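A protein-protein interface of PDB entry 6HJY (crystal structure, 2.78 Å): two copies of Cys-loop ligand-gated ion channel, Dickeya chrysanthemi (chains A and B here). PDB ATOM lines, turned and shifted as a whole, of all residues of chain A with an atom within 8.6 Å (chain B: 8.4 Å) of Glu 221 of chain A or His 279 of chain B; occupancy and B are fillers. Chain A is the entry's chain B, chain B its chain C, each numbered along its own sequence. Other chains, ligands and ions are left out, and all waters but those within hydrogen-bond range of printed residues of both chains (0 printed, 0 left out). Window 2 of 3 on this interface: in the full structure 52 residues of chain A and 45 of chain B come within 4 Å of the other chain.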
ATOM      1  N   SER A 216       3.238  11.062   4.183  1.00  0.00           N
ATOM      2  CA  SER A 216       2.566   9.940   4.849  1.00  0.00           C
ATOM      3  C   SER A 216       3.530   8.841   5.346  1.00  0.00           C
ATOM      4  O   SER A 216       3.093   7.924   6.045  1.00  0.00           O
ATOM      5  CB  SER A 216       1.472   9.356   3.953  1.00  0.00           C
ATOM      6  OG  SER A 216       1.985   8.506   2.938  1.00  0.00           O
ATOM      7  N   VAL A 217       4.831   8.943   4.996  1.00  0.00           N
ATOM      8  CA  VAL A 217       5.885   7.995   5.389  1.00  0.00           C
ATOM      9  C   VAL A 217       6.209   8.077   6.893  1.00  0.00           C
ATOM     10  O   VAL A 217       6.717   7.105   7.455  1.00  0.00           O
ATOM     11  CB  VAL A 217       7.171   8.068   4.506  1.00  0.00           C
ATOM     12  CG1 VAL A 217       6.865   7.724   3.051  1.00  0.00           C
ATOM     13  CG2 VAL A 217       7.879   9.417   4.616  1.00  0.00           C
ATOM     14  N   PHE A 218       5.918   9.234   7.533  1.00  0.00           N
ATOM     15  CA  PHE A 218       6.146   9.495   8.958  1.00  0.00           C
ATOM     16  C   PHE A 218       5.210   8.683   9.855  1.00  0.00           C
ATOM     17  O   PHE A 218       5.501   8.496  11.039  1.00  0.00           O
ATOM     18  CB  PHE A 218       6.030  10.998   9.261  1.00  0.00           C
ATOM     19  CG  PHE A 218       7.200  11.808   8.765  1.00  0.00           C
ATOM     20  CD1 PHE A 218       8.302  12.037   9.580  1.00  0.00           C
ATOM     21  CD2 PHE A 218       7.209  12.331   7.479  1.00  0.00           C
ATOM     22  CE1 PHE A 218       9.394  12.775   9.116  1.00  0.00           C
ATOM     23  CE2 PHE A 218       8.301  13.068   7.015  1.00  0.00           C
ATOM     24  CZ  PHE A 218       9.388  13.282   7.836  1.00  0.00           C
ATOM     25  N   TRP A 219       4.107   8.173   9.275  1.00  0.00           N
ATOM     26  CA  TRP A 219       3.110   7.352   9.955  1.00  0.00           C
ATOM     27  C   TRP A 219       3.531   5.872  10.042  1.00  0.00           C
ATOM     28  O   TRP A 219       2.786   5.063  10.594  1.00  0.00           O
ATOM     29  CB  TRP A 219       1.725   7.546   9.315  1.00  0.00           C
ATOM     30  CG  TRP A 219       1.237   8.965   9.402  1.00  0.00           C
ATOM     31  CD1 TRP A 219       1.356   9.932   8.449  1.00  0.00           C
ATOM     32  CD2 TRP A 219       0.609   9.588  10.533  1.00  0.00           C
ATOM     33  NE1 TRP A 219       0.817  11.115   8.902  1.00  0.00           N
ATOM     34  CE2 TRP A 219       0.350  10.933  10.180  1.00  0.00           C
ATOM     35  CE3 TRP A 219       0.223   9.136  11.807  1.00  0.00           C
ATOM     36  CZ2 TRP A 219      -0.278  11.830  11.055  1.00  0.00           C
ATOM     37  CZ3 TRP A 219      -0.397  10.025  12.674  1.00  0.00           C
ATOM     38  CH2 TRP A 219      -0.643  11.354  12.299  1.00  0.00           C
ATOM     39  N   LEU A 220       4.743   5.534   9.533  1.00  0.00           N
ATOM     40  CA  LEU A 220       5.323   4.188   9.597  1.00  0.00           C
ATOM     41  C   LEU A 220       5.954   3.976  10.975  1.00  0.00           C
ATOM     42  O   LEU A 220       6.570   4.895  11.527  1.00  0.00           O
ATOM     43  CB  LEU A 220       6.355   3.960   8.481  1.00  0.00           C
ATOM     44  CG  LEU A 220       5.800   3.563   7.116  1.00  0.00           C
ATOM     45  CD1 LEU A 220       6.771   3.931   6.016  1.00  0.00           C
ATOM     46  CD2 LEU A 220       5.464   2.069   7.058  1.00  0.00           C
ATOM     47  N   GLU A 221       5.810   2.755  11.514  1.00  0.00           N
ATOM     48  CA  GLU A 221       6.241   2.355  12.852  1.00  0.00           C
ATOM     49  C   GLU A 221       7.759   2.400  13.088  1.00  0.00           C
ATOM     50  O   GLU A 221       8.195   3.103  14.002  1.00  0.00           O
ATOM     51  CB  GLU A 221       5.668   0.967  13.231  1.00  0.00           C
ATOM     52  CG  GLU A 221       4.156   0.821  13.080  1.00  0.00           C
ATOM     53  CD  GLU A 221       3.321   1.842  13.830  1.00  0.00           C
ATOM     54  OE1 GLU A 221       2.782   2.763  13.176  1.00  0.00           O
ATOM     55  OE2 GLU A 221       3.238   1.744  15.075  1.00  0.00           O
ATOM     56  N   SER A 222       8.553   1.652  12.300  1.00  0.00           N
ATOM     57  CA  SER A 222      10.006   1.588  12.488  1.00  0.00           C
ATOM     58  C   SER A 222      10.813   2.498  11.556  1.00  0.00           C
ATOM     59  O   SER A 222      10.294   2.982  10.549  1.00  0.00           O
ATOM     60  CB  SER A 222      10.498   0.143  12.397  1.00  0.00           C
ATOM     61  OG  SER A 222      10.532  -0.330  11.060  1.00  0.00           O
ATOM     62  N   PHE A 223      12.096   2.731  11.920  1.00  0.00           N
ATOM     63  CA  PHE A 223      13.072   3.535  11.178  1.00  0.00           C
ATOM     64  C   PHE A 223      13.407   2.870   9.837  1.00  0.00           C
ATOM     65  O   PHE A 223      13.587   3.569   8.834  1.00  0.00           O
ATOM     66  CB  PHE A 223      14.347   3.740  12.027  1.00  0.00           C
ATOM     67  CG  PHE A 223      15.542   4.351  11.323  1.00  0.00           C
ATOM     68  CD1 PHE A 223      15.563   5.701  10.997  1.00  0.00           C
ATOM     69  CD2 PHE A 223      16.662   3.584  11.025  1.00  0.00           C
ATOM     70  CE1 PHE A 223      16.672   6.269  10.359  1.00  0.00           C
ATOM     71  CE2 PHE A 223      17.773   4.152  10.387  1.00  0.00           C
ATOM     72  CZ  PHE A 223      17.770   5.490  10.060  1.00  0.00           C
ATOM     73  N   SER A 224      13.473   1.517   9.831  1.00  0.00           N
ATOM     74  CA  SER A 224      13.750   0.669   8.663  1.00  0.00           C
ATOM     75  C   SER A 224      12.655   0.817   7.599  1.00  0.00           C
ATOM     76  O   SER A 224      12.963   0.834   6.406  1.00  0.00           O
ATOM     77  CB  SER A 224      13.883  -0.790   9.086  1.00  0.00           C
ATOM     78  OG  SER A 224      14.330  -1.614   8.021  1.00  0.00           O
ATOM     79  N   GLU A 225      11.384   0.953   8.043  1.00  0.00           N
ATOM     80  CA  GLU A 225      10.206   1.127   7.189  1.00  0.00           C
ATOM     81  C   GLU A 225      10.140   2.542   6.615  1.00  0.00           C
ATOM     82  O   GLU A 225       9.934   2.688   5.411  1.00  0.00           O
ATOM     83  CB  GLU A 225       8.914   0.801   7.962  1.00  0.00           C
ATOM     84  CG  GLU A 225       8.711  -0.683   8.223  1.00  0.00           C
ATOM     85  CD  GLU A 225       7.732  -0.997   9.342  1.00  0.00           C
ATOM     86  OE1 GLU A 225       6.583  -0.502   9.293  1.00  0.00           O
ATOM     87  OE2 GLU A 225       8.106  -1.763  10.258  1.00  0.00           O
ATOM     88  N   ARG A 226      10.324   3.577   7.478  1.00  0.00           N
ATOM     89  CA  ARG A 226      10.297   5.006   7.132  1.00  0.00           C
ATOM     90  C   ARG A 226      11.294   5.352   6.028  1.00  0.00           C
ATOM     91  O   ARG A 226      10.925   6.017   5.057  1.00  0.00           O
ATOM     92  CB  ARG A 226      10.600   5.879   8.364  1.00  0.00           C
ATOM     93  CG  ARG A 226       9.436   6.043   9.321  1.00  0.00           C
ATOM     94  CD  ARG A 226       9.700   7.158  10.322  1.00  0.00           C
ATOM     95  NE  ARG A 226      10.783   6.833  11.258  1.00  0.00           N
ATOM     96  CZ  ARG A 226      10.621   6.186  12.411  1.00  0.00           C
ATOM     97  NH1 ARG A 226       9.420   5.753  12.775  1.00  0.00           N
ATOM     98  NH2 ARG A 226      11.661   5.958  13.202  1.00  0.00           N
ATOM     99  N   HIS A 279      16.445   9.097  14.896  1.00  0.00           N
ATOM    100  CA  HIS A 279      17.126   7.851  15.238  1.00  0.00           C
ATOM    101  C   HIS A 279      18.496   8.092  15.880  1.00  0.00           C
ATOM    102  O   HIS A 279      18.645   7.830  17.072  1.00  0.00           O
ATOM    103  CB  HIS A 279      17.223   6.930  14.007  1.00  0.00           C
ATOM    104  CG  HIS A 279      17.137   5.469  14.332  1.00  0.00           C
ATOM    105  ND1 HIS A 279      18.143   4.590  13.974  1.00  0.00           N
ATOM    106  CD2 HIS A 279      16.158   4.782  14.965  1.00  0.00           C
ATOM    107  CE1 HIS A 279      17.747   3.403  14.397  1.00  0.00           C
ATOM    108  NE2 HIS A 279      16.559   3.468  15.001  1.00  0.00           N
ATOM    109  N   SER B 222      -0.739  -6.995   7.503  1.00  0.00           N
ATOM    110  CA  SER B 222      -0.288  -5.836   8.284  1.00  0.00           C
ATOM    111  C   SER B 222      -0.372  -4.498   7.546  1.00  0.00           C
ATOM    112  O   SER B 222      -0.459  -4.467   6.317  1.00  0.00           O
ATOM    113  CB  SER B 222       1.123  -6.068   8.824  1.00  0.00           C
ATOM    114  OG  SER B 222       2.114  -5.922   7.820  1.00  0.00           O
ATOM    115  N   PHE B 223      -0.343  -3.389   8.321  1.00  0.00           N
ATOM    116  CA  PHE B 223      -0.373  -2.002   7.845  1.00  0.00           C
ATOM    117  C   PHE B 223       0.901  -1.679   7.053  1.00  0.00           C
ATOM    118  O   PHE B 223       0.838  -0.927   6.077  1.00  0.00           O
ATOM    119  CB  PHE B 223      -0.548  -1.039   9.041  1.00  0.00           C
ATOM    120  CG  PHE B 223      -0.318   0.436   8.773  1.00  0.00           C
ATOM    121  CD1 PHE B 223      -1.267   1.193   8.099  1.00  0.00           C
ATOM    122  CD2 PHE B 223       0.825   1.075   9.239  1.00  0.00           C
ATOM    123  CE1 PHE B 223      -1.062   2.560   7.865  1.00  0.00           C
ATOM    124  CE2 PHE B 223       1.031   2.441   9.006  1.00  0.00           C
ATOM    125  CZ  PHE B 223       0.083   3.173   8.324  1.00  0.00           C
ATOM    126  N   SER B 224       2.046  -2.272   7.471  1.00  0.00           N
ATOM    127  CA  SER B 224       3.369  -2.130   6.843  1.00  0.00           C
ATOM    128  C   SER B 224       3.365  -2.700   5.419  1.00  0.00           C
ATOM    129  O   SER B 224       4.001  -2.127   4.531  1.00  0.00           O
ATOM    130  CB  SER B 224       4.436  -2.821   7.687  1.00  0.00           C
ATOM    131  OG  SER B 224       5.747  -2.556   7.218  1.00  0.00           O
ATOM    132  N   ARG B 226       0.359  -3.285   3.490  1.00  0.00           N
ATOM    133  CA  ARG B 226      -0.678  -2.543   2.747  1.00  0.00           C
ATOM    134  C   ARG B 226      -0.151  -1.232   2.164  1.00  0.00           C
ATOM    135  O   ARG B 226      -0.452  -0.909   1.013  1.00  0.00           O
ATOM    136  CB  ARG B 226      -1.896  -2.231   3.639  1.00  0.00           C
ATOM    137  CG  ARG B 226      -2.688  -3.449   4.091  1.00  0.00           C
ATOM    138  CD  ARG B 226      -4.067  -3.077   4.611  1.00  0.00           C
ATOM    139  NE  ARG B 226      -4.007  -2.157   5.753  1.00  0.00           N
ATOM    140  CZ  ARG B 226      -3.903  -2.527   7.026  1.00  0.00           C
ATOM    141  NH1 ARG B 226      -3.814  -3.814   7.347  1.00  0.00           N
ATOM    142  NH2 ARG B 226      -3.869  -1.614   7.987  1.00  0.00           N
ATOM    143  N   LEU B 227       0.618  -0.475   2.972  1.00  0.00           N
ATOM    144  CA  LEU B 227       1.178   0.820   2.599  1.00  0.00           C
ATOM    145  C   LEU B 227       2.288   0.710   1.555  1.00  0.00           C
ATOM    146  O   LEU B 227       2.196   1.367   0.517  1.00  0.00           O
ATOM    147  CB  LEU B 227       1.647   1.593   3.849  1.00  0.00           C
ATOM    148  CG  LEU B 227       2.173   3.023   3.631  1.00  0.00           C
ATOM    149  CD1 LEU B 227       1.081   3.955   3.094  1.00  0.00           C
ATOM    150  CD2 LEU B 227       2.729   3.586   4.912  1.00  0.00           C
ATOM    151  N   LEU B 273      -5.713   6.955   1.643  1.00  0.00           N
ATOM    152  CA  LEU B 273      -6.482   7.660   2.677  1.00  0.00           C
ATOM    153  C   LEU B 273      -7.311   6.681   3.522  1.00  0.00           C
ATOM    154  O   LEU B 273      -7.532   6.934   4.708  1.00  0.00           O
ATOM    155  CB  LEU B 273      -7.402   8.740   2.070  1.00  0.00           C
ATOM    156  CG  LEU B 273      -6.742  10.027   1.560  1.00  0.00           C
ATOM    157  CD1 LEU B 273      -7.699  10.806   0.685  1.00  0.00           C
ATOM    158  CD2 LEU B 273      -6.249  10.911   2.712  1.00  0.00           C
ATOM    159  N   LEU B 274      -7.757   5.570   2.905  1.00  0.00           N
ATOM    160  CA  LEU B 274      -8.552   4.513   3.529  1.00  0.00           C
ATOM    161  C   LEU B 274      -7.689   3.656   4.480  1.00  0.00           C
ATOM    162  O   LEU B 274      -8.162   3.306   5.564  1.00  0.00           O
ATOM    163  CB  LEU B 274      -9.208   3.650   2.430  1.00  0.00           C
ATOM    164  CG  LEU B 274     -10.643   3.988   1.967  1.00  0.00           C
ATOM    165  CD1 LEU B 274     -10.716   5.318   1.204  1.00  0.00           C
ATOM    166  CD2 LEU B 274     -11.169   2.909   1.058  1.00  0.00           C
ATOM    167  N   ILE B 275      -6.424   3.343   4.081  1.00  0.00           N
ATOM    168  CA  ILE B 275      -5.455   2.569   4.874  1.00  0.00           C
ATOM    169  C   ILE B 275      -5.082   3.352   6.152  1.00  0.00           C
ATOM    170  O   ILE B 275      -5.061   2.766   7.236  1.00  0.00           O
ATOM    171  CB  ILE B 275      -4.214   2.108   4.029  1.00  0.00           C
ATOM    172  CG1 ILE B 275      -4.623   1.053   2.971  1.00  0.00           C
ATOM    173  CG2 ILE B 275      -3.074   1.557   4.917  1.00  0.00           C
ATOM    174  CD1 ILE B 275      -3.590   0.766   1.838  1.00  0.00           C
ATOM    175  N   ILE B 276      -4.833   4.676   6.017  1.00  0.00           N
ATOM    176  CA  ILE B 276      -4.501   5.585   7.124  1.00  0.00           C
ATOM    177  C   ILE B 276      -5.705   5.718   8.081  1.00  0.00           C
ATOM    178  O   ILE B 276      -5.515   5.725   9.299  1.00  0.00           O
ATOM    179  CB  ILE B 276      -3.967   6.967   6.611  1.00  0.00           C
ATOM    180  CG1 ILE B 276      -2.700   6.797   5.741  1.00  0.00           C
ATOM    181  CG2 ILE B 276      -3.693   7.954   7.773  1.00  0.00           C
ATOM    182  CD1 ILE B 276      -2.399   7.958   4.760  1.00  0.00           C
ATOM    183  N   PHE B 277      -6.939   5.742   7.528  1.00  0.00           N
ATOM    184  CA  PHE B 277      -8.188   5.855   8.294  1.00  0.00           C
ATOM    185  C   PHE B 277      -8.580   4.545   9.036  1.00  0.00           C
ATOM    186  O   PHE B 277      -9.747   4.348   9.383  1.00  0.00           O
ATOM    187  CB  PHE B 277      -9.329   6.372   7.392  1.00  0.00           C
ATOM    188  CG  PHE B 277     -10.298   7.312   8.075  1.00  0.00           C
ATOM    189  CD1 PHE B 277     -10.016   8.669   8.184  1.00  0.00           C
ATOM    190  CD2 PHE B 277     -11.499   6.844   8.591  1.00  0.00           C
ATOM    191  CE1 PHE B 277     -10.911   9.537   8.819  1.00  0.00           C
ATOM    192  CE2 PHE B 277     -12.391   7.711   9.230  1.00  0.00           C
ATOM    193  CZ  PHE B 277     -12.091   9.051   9.335  1.00  0.00           C
ATOM    194  N   ALA B 278      -7.595   3.677   9.309  1.00  0.00           N
ATOM    195  CA  ALA B 278      -7.797   2.421  10.026  1.00  0.00           C
ATOM    196  C   ALA B 278      -6.774   2.260  11.158  1.00  0.00           C
ATOM    197  O   ALA B 278      -7.149   1.863  12.261  1.00  0.00           O
ATOM    198  CB  ALA B 278      -7.694   1.254   9.056  1.00  0.00           C
ATOM    199  N   HIS B 279      -5.493   2.591  10.877  1.00  0.00           N
ATOM    200  CA  HIS B 279      -4.349   2.495  11.786  1.00  0.00           C
ATOM    201  C   HIS B 279      -4.374   3.576  12.878  1.00  0.00           C
ATOM    202  O   HIS B 279      -4.717   3.257  14.019  1.00  0.00           O
ATOM    203  CB  HIS B 279      -3.042   2.527  10.970  1.00  0.00           C
ATOM    204  CG  HIS B 279      -1.826   2.042  11.703  1.00  0.00           C
ATOM    205  ND1 HIS B 279      -1.665   0.710  12.042  1.00  0.00           N
ATOM    206  CD2 HIS B 279      -0.717   2.723  12.070  1.00  0.00           C
ATOM    207  CE1 HIS B 279      -0.488   0.633  12.637  1.00  0.00           C
ATOM    208  NE2 HIS B 279       0.123   1.816  12.675  1.00  0.00           N
ATOM    209  N   HIS B 280      -4.035   4.843  12.537  1.00  0.00           N
ATOM    210  CA  HIS B 280      -4.021   5.968  13.480  1.00  0.00           C
ATOM    211  C   HIS B 280      -5.391   6.632  13.560  1.00  0.00           C
ATOM    212  O   HIS B 280      -5.704   7.296  14.547  1.00  0.00           O
ATOM    213  CB  HIS B 280      -2.948   7.003  13.086  1.00  0.00           C
ATOM    214  CG  HIS B 280      -1.594   6.732  13.672  1.00  0.00           C
ATOM    215  ND1 HIS B 280      -0.649   5.986  12.994  1.00  0.00           N
ATOM    216  CD2 HIS B 280      -1.070   7.133  14.854  1.00  0.00           C
ATOM    217  CE1 HIS B 280       0.411   5.950  13.782  1.00  0.00           C
ATOM    218  NE2 HIS B 280       0.207   6.625  14.912  1.00  0.00           N
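OE1 of Glu 221 of chain A is in hydrogen-bond range of NE2 of His 279 of chain B (2.9 Å). The side-chain hydroxyl of Ser 224 of chain B is in hydrogen-bond range of the side-chain carboxylate of Glu 225 of chain A (3.0 Å).
The backbone carbonyl oxygen (O) of Leu 220 of chain A is in hydrogen-bond range of the guanidinium group (NH1) of Arg 226 of chain A. NH1 of Arg 226 of chain A is in hydrogen-bond range of O of Glu 221 of chain A. OG of Ser 222 of chain A lies within hydrogen-bond range of OE2 of Glu 225 of chain A, 2.9 Å away.
Among the printed residues, pairs that only touch across the chains: Trp 219 of chain A with His 280 of chain B (3.5 Å), Trp 219 of chain A with Phe 223 of chain B (3.5 Å) and Leu 220 of chain A with Leu 227 of chain B (3.8 Å).
Printed residues of chain B within 4 Å of Trp 219 of chain A: Phe 223 and His 280. Printed residues of chain B within 4 Å of Leu 220 of chain A: Leu 227 (3.8 Å). Printed residues of chain B within 4 Å of Glu 221 of chain A: His 279. Of the printed residues of chain B, Glu 225 of chain A touches Ser 224. Of the printed residues of chain A, Phe 223 of chain B touches Trp 219 (3.5 Å). Arg 226 of chain B touches none of the printed residues of chain A. Of the printed residues of chain A, Leu 227 of chain B touches Leu 220. Leu 273 of chain B touches none of the printed residues of chain A. No residue of chain A comes within 4 Å of Ala 278 of chain B. Printed residues of chain A within 4 Å of His 279 of chain B: Glu 221 (2.9 Å). The nearest residue of chain A that does not touch His 279 of chain B is Trp 219 of chain A (4.5 Å). The nearest printed residue of chain B that does not touch Leu 220 of chain A is Ser 224 of chain B (4.6 Å).
Of the 13 printed residues of chain B, 5 touch a printed residue of chain A. Hydrophobic or aromatic side chains of chain B that line the printed part of chain A: Phe 223, Leu 227, His 279 and His 280. Along chain B the printed residues that touch a printed residue of chain A span positions 223 to 280. Printed residues of chain A that touch a printed residue of chain B: Trp 219, Leu 220, Glu 221 and Glu 225. Along chain A the printed residues that touch a printed residue of chain B span positions 219 to 225.
Positions printed for both chains: 222, 223, 224, 226 and 279. Of the 5 pairs that touch across the chains among the printed residues, none has its exchanged pair printed and touching as well.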
